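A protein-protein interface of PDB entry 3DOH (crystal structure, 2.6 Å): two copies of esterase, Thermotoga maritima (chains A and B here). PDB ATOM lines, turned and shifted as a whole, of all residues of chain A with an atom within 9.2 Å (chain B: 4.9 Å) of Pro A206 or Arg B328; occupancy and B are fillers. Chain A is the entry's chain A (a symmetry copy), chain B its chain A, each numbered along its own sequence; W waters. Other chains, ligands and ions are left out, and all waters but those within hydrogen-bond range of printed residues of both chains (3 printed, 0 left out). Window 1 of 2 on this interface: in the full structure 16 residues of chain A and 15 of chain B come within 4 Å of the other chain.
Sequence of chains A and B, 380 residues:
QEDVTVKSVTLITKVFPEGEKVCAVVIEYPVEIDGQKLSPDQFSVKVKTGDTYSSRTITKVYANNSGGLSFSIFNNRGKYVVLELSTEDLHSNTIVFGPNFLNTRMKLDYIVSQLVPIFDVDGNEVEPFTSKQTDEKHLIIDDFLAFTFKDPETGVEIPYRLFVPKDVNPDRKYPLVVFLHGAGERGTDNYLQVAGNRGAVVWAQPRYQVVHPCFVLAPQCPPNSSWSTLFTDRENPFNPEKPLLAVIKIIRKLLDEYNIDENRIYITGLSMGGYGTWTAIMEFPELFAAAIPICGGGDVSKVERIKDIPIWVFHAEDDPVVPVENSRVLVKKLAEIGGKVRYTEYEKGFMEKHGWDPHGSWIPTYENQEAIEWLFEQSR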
ATOM      1  N   LYS A  14     -20.024  19.546 -19.872  1.00  0.00           N
ATOM      2  CA  LYS A  14     -19.466  20.632 -19.121  1.00  0.00           C
ATOM      3  C   LYS A  14     -20.243  21.876 -19.550  1.00  0.00           C
ATOM      4  O   LYS A  14     -20.672  21.978 -20.727  1.00  0.00           O
ATOM      5  CB  LYS A  14     -18.004  20.731 -19.507  1.00  0.00           C
ATOM      6  CG  LYS A  14     -17.199  21.742 -18.748  1.00  0.00           C
ATOM      7  CD  LYS A  14     -16.091  22.231 -19.632  1.00  0.00           C
ATOM      8  CE  LYS A  14     -14.891  22.670 -18.846  1.00  0.00           C
ATOM      9  NZ  LYS A  14     -14.128  21.485 -18.363  1.00  0.00           N
ATOM     10  N   LEU A 139     -20.081  17.684 -15.331  1.00  0.00           N
ATOM     11  CA  LEU A 139     -18.940  18.187 -14.577  1.00  0.00           C
ATOM     12  C   LEU A 139     -19.241  19.549 -13.961  1.00  0.00           C
ATOM     13  O   LEU A 139     -19.128  20.580 -14.623  1.00  0.00           O
ATOM     14  CB  LEU A 139     -17.703  18.279 -15.474  1.00  0.00           C
ATOM     15  CG  LEU A 139     -16.833  17.023 -15.560  1.00  0.00           C
ATOM     16  CD1 LEU A 139     -15.640  17.257 -16.474  1.00  0.00           C
ATOM     17  CD2 LEU A 139     -16.377  16.589 -14.176  1.00  0.00           C
ATOM     18  N   ILE A 140     -19.628  19.545 -12.689  1.00  0.00           N
ATOM     19  CA  ILE A 140     -19.913  20.781 -11.970  1.00  0.00           C
ATOM     20  C   ILE A 140     -21.408  20.940 -11.717  1.00  0.00           C
ATOM     21  O   ILE A 140     -21.820  21.477 -10.690  1.00  0.00           O
ATOM     22  CB  ILE A 140     -19.398  22.012 -12.740  1.00  0.00           C
ATOM     23  CG1 ILE A 140     -17.899  21.876 -13.021  1.00  0.00           C
ATOM     24  CG2 ILE A 140     -19.686  23.286 -11.961  1.00  0.00           C
ATOM     25  CD1 ILE A 140     -17.029  22.065 -11.797  1.00  0.00           C
ATOM     26  N   ASP A 143     -22.283  18.735  -8.721  1.00  0.00           N
ATOM     27  CA  ASP A 143     -22.071  19.189  -7.333  1.00  0.00           C
ATOM     28  C   ASP A 143     -23.213  19.965  -6.705  1.00  0.00           C
ATOM     29  O   ASP A 143     -23.146  20.274  -5.515  1.00  0.00           O
ATOM     30  CB  ASP A 143     -20.814  20.046  -7.172  1.00  0.00           C
ATOM     31  CG  ASP A 143     -19.591  19.382  -7.718  1.00  0.00           C
ATOM     32  OD1 ASP A 143     -19.294  18.254  -7.275  1.00  0.00           O
ATOM     33  OD2 ASP A 143     -18.923  19.986  -8.596  1.00  0.00           O
ATOM     34  N   PHE A 163     -25.509  24.680  -4.556  1.00  0.00           N
ATOM     35  CA  PHE A 163     -24.096  24.262  -4.356  1.00  0.00           C
ATOM     36  C   PHE A 163     -23.701  24.558  -2.922  1.00  0.00           C
ATOM     37  O   PHE A 163     -23.851  25.663  -2.448  1.00  0.00           O
ATOM     38  CB  PHE A 163     -23.151  25.016  -5.324  1.00  0.00           C
ATOM     39  CG  PHE A 163     -21.651  24.708  -5.164  1.00  0.00           C
ATOM     40  CD1 PHE A 163     -21.036  23.678  -5.920  1.00  0.00           C
ATOM     41  CD2 PHE A 163     -20.838  25.512  -4.352  1.00  0.00           C
ATOM     42  CE1 PHE A 163     -19.623  23.433  -5.851  1.00  0.00           C
ATOM     43  CE2 PHE A 163     -19.432  25.274  -4.246  1.00  0.00           C
ATOM     44  CZ  PHE A 163     -18.826  24.218  -5.005  1.00  0.00           C
ATOM     45  N   LYS A 166     -17.178  22.909  -0.116  1.00  0.00           N
ATOM     46  CA  LYS A 166     -16.549  21.750   0.489  1.00  0.00           C
ATOM     47  C   LYS A 166     -15.241  22.081   1.184  1.00  0.00           C
ATOM     48  O   LYS A 166     -14.500  22.973   0.750  1.00  0.00           O
ATOM     49  CB  LYS A 166     -16.308  20.649  -0.549  1.00  0.00           C
ATOM     50  CG  LYS A 166     -15.956  21.138  -1.985  1.00  0.00           C
ATOM     51  CD  LYS A 166     -14.820  20.317  -2.655  1.00  0.00           C
ATOM     52  CE  LYS A 166     -14.848  18.833  -2.248  1.00  0.00           C
ATOM     53  NZ  LYS A 166     -13.768  17.974  -2.924  1.00  0.00           N
ATOM     54  N   VAL A 201     -22.941  28.165 -12.454  1.00  0.00           N
ATOM     55  CA  VAL A 201     -21.848  27.262 -12.320  1.00  0.00           C
ATOM     56  C   VAL A 201     -20.500  27.981 -12.169  1.00  0.00           C
ATOM     57  O   VAL A 201     -19.585  27.498 -11.495  1.00  0.00           O
ATOM     58  CB  VAL A 201     -21.941  26.373 -13.579  1.00  0.00           C
ATOM     59  CG1 VAL A 201     -20.709  26.431 -14.443  1.00  0.00           C
ATOM     60  CG2 VAL A 201     -22.499  24.995 -13.259  1.00  0.00           C
ATOM     61  N   VAL A 202     -20.372  29.162 -12.750  1.00  0.00           N
ATOM     62  CA  VAL A 202     -19.100  29.908 -12.661  1.00  0.00           C
ATOM     63  C   VAL A 202     -18.713  30.076 -11.183  1.00  0.00           C
ATOM     64  O   VAL A 202     -17.570  29.814 -10.800  1.00  0.00           O
ATOM     65  CB  VAL A 202     -19.162  31.265 -13.447  1.00  0.00           C
ATOM     66  CG1 VAL A 202     -20.239  32.202 -12.872  1.00  0.00           C
ATOM     67  CG2 VAL A 202     -17.808  31.929 -13.488  1.00  0.00           C
ATOM     68  N   TRP A 203     -19.694  30.432 -10.352  1.00  0.00           N
ATOM     69  CA  TRP A 203     -19.428  30.668  -8.960  1.00  0.00           C
ATOM     70  C   TRP A 203     -18.969  29.379  -8.317  1.00  0.00           C
ATOM     71  O   TRP A 203     -18.388  29.376  -7.257  1.00  0.00           O
ATOM     72  CB  TRP A 203     -20.665  31.198  -8.294  1.00  0.00           C
ATOM     73  CG  TRP A 203     -21.376  32.241  -9.172  1.00  0.00           C
ATOM     74  CD1 TRP A 203     -22.490  32.038  -9.954  1.00  0.00           C
ATOM     75  CD2 TRP A 203     -20.998  33.613  -9.358  1.00  0.00           C
ATOM     76  NE1 TRP A 203     -22.816  33.199 -10.610  1.00  0.00           N
ATOM     77  CE2 TRP A 203     -21.915  34.178 -10.263  1.00  0.00           C
ATOM     78  CE3 TRP A 203     -19.956  34.408  -8.867  1.00  0.00           C
ATOM     79  CZ2 TRP A 203     -21.832  35.518 -10.674  1.00  0.00           C
ATOM     80  CZ3 TRP A 203     -19.875  35.738  -9.264  1.00  0.00           C
ATOM     81  CH2 TRP A 203     -20.801  36.275 -10.163  1.00  0.00           C
ATOM     82  N   ALA A 204     -19.181  28.271  -9.003  1.00  0.00           N
ATOM     83  CA  ALA A 204     -18.927  26.992  -8.381  1.00  0.00           C
ATOM     84  C   ALA A 204     -17.642  26.377  -8.883  1.00  0.00           C
ATOM     85  O   ALA A 204     -17.203  25.356  -8.357  1.00  0.00           O
ATOM     86  CB  ALA A 204     -20.128  26.046  -8.573  1.00  0.00           C
ATOM     87  N   GLN A 205     -17.020  27.011  -9.866  1.00  0.00           N
ATOM     88  CA  GLN A 205     -15.701  26.570 -10.354  1.00  0.00           C
ATOM     89  C   GLN A 205     -14.620  26.595  -9.264  1.00  0.00           C
ATOM     90  O   GLN A 205     -14.559  27.535  -8.501  1.00  0.00           O
ATOM     91  CB  GLN A 205     -15.312  27.383 -11.596  1.00  0.00           C
ATOM     92  CG  GLN A 205     -15.990  26.836 -12.901  1.00  0.00           C
ATOM     93  CD  GLN A 205     -15.840  27.763 -14.096  1.00  0.00           C
ATOM     94  OE1 GLN A 205     -16.481  27.546 -15.139  1.00  0.00           O
ATOM     95  NE2 GLN A 205     -14.990  28.819 -13.968  1.00  0.00           N
ATOM     96  N   PRO A 206     -13.831  25.514  -9.102  1.00  0.00           N
ATOM     97  CA  PRO A 206     -12.627  25.583  -8.228  1.00  0.00           C
ATOM     98  C   PRO A 206     -11.805  26.878  -8.257  1.00  0.00           C
ATOM     99  O   PRO A 206     -11.489  27.409  -7.194  1.00  0.00           O
ATOM    100  CB  PRO A 206     -11.804  24.388  -8.682  1.00  0.00           C
ATOM    101  CG  PRO A 206     -12.866  23.383  -9.019  1.00  0.00           C
ATOM    102  CD  PRO A 206     -14.014  24.146  -9.636  1.00  0.00           C
ATOM    103  N   ARG A 207     -11.515  27.437  -9.424  1.00  0.00           N
ATOM    104  CA  ARG A 207     -10.720  28.708  -9.462  1.00  0.00           C
ATOM    105  C   ARG A 207     -11.278  29.815  -8.553  1.00  0.00           C
ATOM    106  O   ARG A 207     -10.512  30.611  -7.988  1.00  0.00           O
ATOM    107  CB  ARG A 207     -10.527  29.239 -10.899  1.00  0.00           C
ATOM    108  CG  ARG A 207     -11.836  29.578 -11.645  1.00  0.00           C
ATOM    109  CD  ARG A 207     -11.590  30.063 -13.072  1.00  0.00           C
ATOM    110  NE  ARG A 207     -10.606  29.190 -13.677  1.00  0.00           N
ATOM    111  CZ  ARG A 207     -10.927  28.101 -14.370  1.00  0.00           C
ATOM    112  NH1 ARG A 207     -12.220  27.808 -14.554  1.00  0.00           N
ATOM    113  NH2 ARG A 207      -9.966  27.319 -14.891  1.00  0.00           N
ATOM    114  N   TYR A 208     -12.610  29.867  -8.425  1.00  0.00           N
ATOM    115  CA  TYR A 208     -13.216  30.883  -7.592  1.00  0.00           C
ATOM    116  C   TYR A 208     -13.493  30.380  -6.201  1.00  0.00           C
ATOM    117  O   TYR A 208     -13.267  31.097  -5.213  1.00  0.00           O
ATOM    118  CB  TYR A 208     -14.481  31.466  -8.245  1.00  0.00           C
ATOM    119  CG  TYR A 208     -14.200  32.074  -9.564  1.00  0.00           C
ATOM    120  CD1 TYR A 208     -13.278  33.144  -9.687  1.00  0.00           C
ATOM    121  CD2 TYR A 208     -14.785  31.569 -10.716  1.00  0.00           C
ATOM    122  CE1 TYR A 208     -12.987  33.701 -10.912  1.00  0.00           C
ATOM    123  CE2 TYR A 208     -14.503  32.136 -11.974  1.00  0.00           C
ATOM    124  CZ  TYR A 208     -13.596  33.195 -12.049  1.00  0.00           C
ATOM    125  OH  TYR A 208     -13.292  33.729 -13.260  1.00  0.00           O
ATOM    126  N   GLN A 209     -13.977  29.149  -6.102  1.00  0.00           N
ATOM    127  CA  GLN A 209     -14.330  28.590  -4.791  1.00  0.00           C
ATOM    128  C   GLN A 209     -13.207  28.638  -3.775  1.00  0.00           C
ATOM    129  O   GLN A 209     -13.424  28.884  -2.612  1.00  0.00           O
ATOM    130  CB  GLN A 209     -14.764  27.155  -4.952  1.00  0.00           C
ATOM    131  CG  GLN A 209     -16.153  27.089  -5.443  1.00  0.00           C
ATOM    132  CD  GLN A 209     -17.113  27.583  -4.403  1.00  0.00           C
ATOM    133  OE1 GLN A 209     -16.886  27.404  -3.195  1.00  0.00           O
ATOM    134  NE2 GLN A 209     -18.208  28.207  -4.857  1.00  0.00           N
ATOM    135  N   VAL A 210     -11.999  28.393  -4.253  1.00  0.00           N
ATOM    136  CA  VAL A 210     -10.804  28.307  -3.446  1.00  0.00           C
ATOM    137  C   VAL A 210     -10.374  29.677  -2.919  1.00  0.00           C
ATOM    138  O   VAL A 210      -9.647  29.769  -1.915  1.00  0.00           O
ATOM    139  CB  VAL A 210      -9.697  27.678  -4.307  1.00  0.00           C
ATOM    140  CG1 VAL A 210      -8.814  28.772  -4.992  1.00  0.00           C
ATOM    141  CG2 VAL A 210      -8.915  26.731  -3.505  1.00  0.00           C
ATOM    142  N   VAL A 211     -10.832  30.756  -3.567  1.00  0.00           N
ATOM    143  CA  VAL A 211     -10.629  32.106  -2.991  1.00  0.00           C
ATOM    144  C   VAL A 211     -11.876  32.732  -2.358  1.00  0.00           C
ATOM    145  O   VAL A 211     -11.758  33.591  -1.493  1.00  0.00           O
ATOM    146  CB  VAL A 211      -9.868  33.094  -3.948  1.00  0.00           C
ATOM    147  CG1 VAL A 211      -8.560  32.487  -4.358  1.00  0.00           C
ATOM    148  CG2 VAL A 211     -10.656  33.369  -5.175  1.00  0.00           C
ATOM    149  N   HIS A 212     -13.052  32.298  -2.799  1.00  0.00           N
ATOM    150  CA  HIS A 212     -14.308  32.786  -2.243  1.00  0.00           C
ATOM    151  C   HIS A 212     -15.351  31.675  -2.178  1.00  0.00           C
ATOM    152  O   HIS A 212     -16.312  31.669  -2.945  1.00  0.00           O
ATOM    153  CB  HIS A 212     -14.840  33.959  -3.068  1.00  0.00           C
ATOM    154  CG  HIS A 212     -13.794  34.968  -3.426  1.00  0.00           C
ATOM    155  ND1 HIS A 212     -13.170  34.991  -4.656  1.00  0.00           N
ATOM    156  CD2 HIS A 212     -13.262  35.991  -2.716  1.00  0.00           C
ATOM    157  CE1 HIS A 212     -12.300  35.984  -4.687  1.00  0.00           C
ATOM    158  NE2 HIS A 212     -12.336  36.607  -3.523  1.00  0.00           N
ATOM    159  N   PRO A 213     -15.153  30.738  -1.258  1.00  0.00           N
ATOM    160  CA  PRO A 213     -16.197  29.768  -0.909  1.00  0.00           C
ATOM    161  C   PRO A 213     -17.503  30.455  -0.528  1.00  0.00           C
ATOM    162  O   PRO A 213     -17.488  31.600  -0.075  1.00  0.00           O
ATOM    163  CB  PRO A 213     -15.608  29.046   0.304  1.00  0.00           C
ATOM    164  CG  PRO A 213     -14.699  30.048   0.924  1.00  0.00           C
ATOM    165  CD  PRO A 213     -14.117  30.836  -0.215  1.00  0.00           C
ATOM    166  N   CYS A 214     -18.620  29.757  -0.708  1.00  0.00           N
ATOM    167  CA  CYS A 214     -19.626  30.159  -1.684  1.00  0.00           C
ATOM    168  C   CYS A 214     -20.721  29.105  -1.815  1.00  0.00           C
ATOM    169  O   CYS A 214     -20.458  27.968  -2.207  1.00  0.00           O
ATOM    170  CB  CYS A 214     -18.980  30.417  -3.046  1.00  0.00           C
ATOM    171  SG  CYS A 214     -20.115  31.043  -4.306  1.00  0.00           S
ATOM    172  N   GLU B 317      -5.376  25.433 -15.463  1.00  0.00           N
ATOM    173  CA  GLU B 317      -6.198  24.285 -15.070  1.00  0.00           C
ATOM    174  C   GLU B 317      -5.721  22.944 -15.635  1.00  0.00           C
ATOM    175  O   GLU B 317      -5.703  21.928 -14.929  1.00  0.00           O
ATOM    176  CB  GLU B 317      -7.625  24.525 -15.507  1.00  0.00           C
ATOM    177  CG  GLU B 317      -8.579  23.482 -14.964  1.00  0.00           C
ATOM    178  CD  GLU B 317      -8.630  22.234 -15.828  1.00  0.00           C
ATOM    179  OE1 GLU B 317      -8.140  22.262 -16.977  1.00  0.00           O
ATOM    180  OE2 GLU B 317      -9.145  21.215 -15.359  1.00  0.00           O
ATOM    181  N   VAL B 324      -2.655  21.492 -11.333  1.00  0.00           N
ATOM    182  CA  VAL B 324      -3.082  22.839 -10.908  1.00  0.00           C
ATOM    183  C   VAL B 324      -3.420  22.801  -9.406  1.00  0.00           C
ATOM    184  O   VAL B 324      -3.375  23.835  -8.697  1.00  0.00           O
ATOM    185  CB  VAL B 324      -4.283  23.344 -11.766  1.00  0.00           C
ATOM    186  CG1 VAL B 324      -5.496  22.390 -11.643  1.00  0.00           C
ATOM    187  CG2 VAL B 324      -4.690  24.770 -11.420  1.00  0.00           C
ATOM    188  N   GLU B 325      -3.749  21.594  -8.919  1.00  0.00           N
ATOM    189  CA  GLU B 325      -4.093  21.410  -7.503  1.00  0.00           C
ATOM    190  C   GLU B 325      -2.958  21.921  -6.591  1.00  0.00           C
ATOM    191  O   GLU B 325      -3.194  22.399  -5.497  1.00  0.00           O
ATOM    192  CB  GLU B 325      -4.451  19.946  -7.236  1.00  0.00           C
ATOM    193  CG  GLU B 325      -4.510  19.558  -5.769  1.00  0.00           C
ATOM    194  CD  GLU B 325      -5.881  19.853  -5.123  1.00  0.00           C
ATOM    195  OE1 GLU B 325      -6.524  20.914  -5.442  1.00  0.00           O
ATOM    196  OE2 GLU B 325      -6.314  18.997  -4.292  1.00  0.00           O
ATOM    197  N   ASN B 326      -1.726  21.825  -7.072  1.00  0.00           N
ATOM    198  CA  ASN B 326      -0.595  22.389  -6.404  1.00  0.00           C
ATOM    199  C   ASN B 326      -0.746  23.874  -6.028  1.00  0.00           C
ATOM    200  O   ASN B 326      -0.347  24.273  -4.941  1.00  0.00           O
ATOM    201  CB  ASN B 326       0.609  22.190  -7.287  1.00  0.00           C
ATOM    202  CG  ASN B 326       1.316  20.887  -7.023  1.00  0.00           C
ATOM    203  OD1 ASN B 326       2.212  20.844  -6.199  1.00  0.00           O
ATOM    204  ND2 ASN B 326       0.944  19.835  -7.719  1.00  0.00           N
ATOM    205  N   SER B 327      -1.305  24.697  -6.912  1.00  0.00           N
ATOM    206  CA  SER B 327      -1.586  26.102  -6.570  1.00  0.00           C
ATOM    207  C   SER B 327      -2.865  26.230  -5.752  1.00  0.00           C
ATOM    208  O   SER B 327      -2.885  26.940  -4.742  1.00  0.00           O
ATOM    209  CB  SER B 327      -1.722  26.967  -7.815  1.00  0.00           C
ATOM    210  OG  SER B 327      -0.456  27.229  -8.330  1.00  0.00           O
ATOM    211  N   ARG B 328      -3.915  25.539  -6.184  1.00  0.00           N
ATOM    212  CA  ARG B 328      -5.200  25.562  -5.460  1.00  0.00           C
ATOM    213  C   ARG B 328      -5.079  25.286  -3.983  1.00  0.00           C
ATOM    214  O   ARG B 328      -5.734  25.971  -3.176  1.00  0.00           O
ATOM    215  CB  ARG B 328      -6.234  24.602  -6.040  1.00  0.00           C
ATOM    216  CG  ARG B 328      -6.752  25.027  -7.347  1.00  0.00           C
ATOM    217  CD  ARG B 328      -7.422  23.913  -7.942  1.00  0.00           C
ATOM    218  NE  ARG B 328      -7.885  24.196  -9.280  1.00  0.00           N
ATOM    219  CZ  ARG B 328      -8.675  23.389  -9.973  1.00  0.00           C
ATOM    220  NH1 ARG B 328      -9.118  22.265  -9.422  1.00  0.00           N
ATOM    221  NH2 ARG B 328      -9.016  23.705 -11.216  1.00  0.00           N
ATOM    222  N   VAL B 329      -4.246  24.309  -3.617  1.00  0.00           N
ATOM    223  CA  VAL B 329      -4.129  23.997  -2.209  1.00  0.00           C
ATOM    224  C   VAL B 329      -3.507  25.146  -1.408  1.00  0.00           C
ATOM    225  O   VAL B 329      -4.044  25.485  -0.364  1.00  0.00           O
ATOM    226  CB  VAL B 329      -3.484  22.608  -1.916  1.00  0.00           C
ATOM    227  CG1 VAL B 329      -2.000  22.585  -2.346  1.00  0.00           C
ATOM    228  CG2 VAL B 329      -3.633  22.285  -0.453  1.00  0.00           C
ATOM    229  N   LEU B 330      -2.419  25.764  -1.890  1.00  0.00           N
ATOM    230  CA  LEU B 330      -1.840  26.891  -1.165  1.00  0.00           C
ATOM    231  C   LEU B 330      -2.839  28.046  -1.097  1.00  0.00           C
ATOM    232  O   LEU B 330      -3.068  28.643  -0.035  1.00  0.00           O
ATOM    233  CB  LEU B 330      -0.540  27.370  -1.810  1.00  0.00           C
ATOM    234  CG  LEU B 330       0.780  26.580  -1.728  1.00  0.00           C
ATOM    235  CD1 LEU B 330       0.869  25.623  -0.537  1.00  0.00           C
ATOM    236  CD2 LEU B 330       0.998  25.827  -3.010  1.00  0.00           C
ATOM    237  N   VAL B 331      -3.454  28.353  -2.233  1.00  0.00           N
ATOM    238  CA  VAL B 331      -4.382  29.489  -2.284  1.00  0.00           C
ATOM    239  C   VAL B 331      -5.548  29.301  -1.310  1.00  0.00           C
ATOM    240  O   VAL B 331      -5.880  30.234  -0.550  1.00  0.00           O
ATOM    241  CB  VAL B 331      -4.916  29.744  -3.694  1.00  0.00           C
ATOM    242  CG1 VAL B 331      -5.937  30.787  -3.642  1.00  0.00           C
ATOM    243  CG2 VAL B 331      -3.808  30.166  -4.589  1.00  0.00           C
ATOM    244  N   LYS B 332      -6.162  28.110  -1.317  1.00  0.00           N
ATOM    245  CA  LYS B 332      -7.278  27.800  -0.404  1.00  0.00           C
ATOM    246  C   LYS B 332      -6.928  28.144   1.025  1.00  0.00           C
ATOM    247  O   LYS B 332      -7.673  28.883   1.687  1.00  0.00           O
ATOM    248  CB  LYS B 332      -7.681  26.331  -0.471  1.00  0.00           C
ATOM    249  CG  LYS B 332      -9.094  26.008   0.029  1.00  0.00           C
ATOM    250  CD  LYS B 332      -9.388  24.493  -0.188  1.00  0.00           C
ATOM    251  CE  LYS B 332     -10.837  24.057   0.116  1.00  0.00           C
ATOM    252  NZ  LYS B 332     -11.379  24.628   1.371  1.00  0.00           N
ATOM    253  N   TYR B 343      -5.447  35.011  -7.159  1.00  0.00           N
ATOM    254  CA  TYR B 343      -5.382  33.780  -7.903  1.00  0.00           C
ATOM    255  C   TYR B 343      -6.179  33.898  -9.173  1.00  0.00           C
ATOM    256  O   TYR B 343      -7.411  34.058  -9.144  1.00  0.00           O
ATOM    257  CB  TYR B 343      -5.921  32.601  -7.086  1.00  0.00           C
ATOM    258  CG  TYR B 343      -5.713  31.271  -7.745  1.00  0.00           C
ATOM    259  CD1 TYR B 343      -4.448  30.883  -8.221  1.00  0.00           C
ATOM    260  CD2 TYR B 343      -6.763  30.393  -7.879  1.00  0.00           C
ATOM    261  CE1 TYR B 343      -4.269  29.650  -8.848  1.00  0.00           C
ATOM    262  CE2 TYR B 343      -6.603  29.160  -8.473  1.00  0.00           C
ATOM    263  CZ  TYR B 343      -5.375  28.772  -8.959  1.00  0.00           C
ATOM    264  OH  TYR B 343      -5.264  27.505  -9.570  1.00  0.00           O
ATOM    265  N   GLU B 345      -6.566  31.468 -12.366  1.00  0.00           N
ATOM    266  CA  GLU B 345      -6.335  30.131 -12.910  1.00  0.00           C
ATOM    267  C   GLU B 345      -6.890  30.053 -14.306  1.00  0.00           C
ATOM    268  O   GLU B 345      -8.119  30.009 -14.495  1.00  0.00           O
ATOM    269  CB  GLU B 345      -6.996  29.070 -12.068  1.00  0.00           C
ATOM    270  CG  GLU B 345      -6.751  27.646 -12.543  1.00  0.00           C
ATOM    271  CD  GLU B 345      -7.577  26.611 -11.764  1.00  0.00           C
ATOM    272  OE1 GLU B 345      -7.490  26.558 -10.515  1.00  0.00           O
ATOM    273  OE2 GLU B 345      -8.339  25.849 -12.401  1.00  0.00           O
HETATM  274  O   HOH W   1     -10.398  29.718   0.733  1.00  0.00           O
HETATM  275  O   HOH W   2      -9.583  32.855  -9.448  1.00  0.00           O
HETATM  276  O   HOH W   3     -12.474  26.789  -0.406  1.00  0.00           O
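Asp A143 touches none of the printed residues of chain B.
Pro A206 touches just one residue of chain B: Arg B328 (3.5 Å).
Of the printed residues of chain B, Arg A207 touches Glu B317 (3.7 Å), Tyr B343 (3.8 Å) and Glu B345 (2.7 Å).
Gln A209 touches none of the printed residues of chain B.
Of the printed residues of chain B, Val A210 touches Arg B328, Val B331, Lys B332 and Tyr B343.
No residue of chain A comes within 4 Å of Ser B327.
Arg B328 touches just these residues of chain A: Pro A206 and Val A210.
No residue of chain A comes within 4 Å of Val B329.
Printed residues of chain A within 4 Å of Glu B345: Arg A207.
The nearest residue of chain A that does not touch Arg B328 is Arg A207 (4.8 Å).
The nearest printed residue of chain B that does not touch Val A211 is Lys B332 (5.6 Å).
Lys A166 touches Lys B332 (O to NZ, 3.6 Å).
Arg B328 touches Pro A206.
CB of Glu B317 touches NH2 of Arg A207, at 3.7 Å.
Arg A207 touches Tyr B343 (O to CD2, 3.8 Å).
Val A210 touches Arg B328.
CG1 of Val A210 touches CG1 of Val B331 (3.8 Å).
Lys B332 touches Val A210.
Tyr B343 touches Val A210.
Val A211 touches Val B331 (CG1 to CG1, 3.2 Å).
Val A211 touches Tyr B343.
The side-chain carboxylate (OE2) of Glu B345 is in salt-bridge range of the guanidinium group (NH2) of Arg A207.
The side-chain amide nitrogen of Gln A205 sits close to the guanidinium group of Arg A207 (3.0 Å).
NH2 of Arg B328 lies within salt-bridge range of OE2 of Glu B345, at 2.5 Å.
OE1 of Glu B345 sits at hydrogen-bond distance from OH of Tyr B343, 2.6 Å away.
Of the 12 printed residues of chain B, 6 touch a printed residue of chain A.
Hydrophobic or aromatic side chains of chain B within 4 Å of the printed part of chain A: Val B331 and Tyr B343.
Water W2 lies within hydrogen-bond range of O of Tyr B343 and O of Arg A207.
Water W1 lies within hydrogen-bond range of O of Val A210 (2.8 Å) and O of Lys B332 (3.0 Å).
Water W3 bridges NZ of Lys B332 (3.0 Å) and O of Gln A209 (3.2 Å).
No position is printed for both chains.
Of the 11 pairs that touch across the chains among the printed residues, none has its exchanged pair printed and touching as well.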
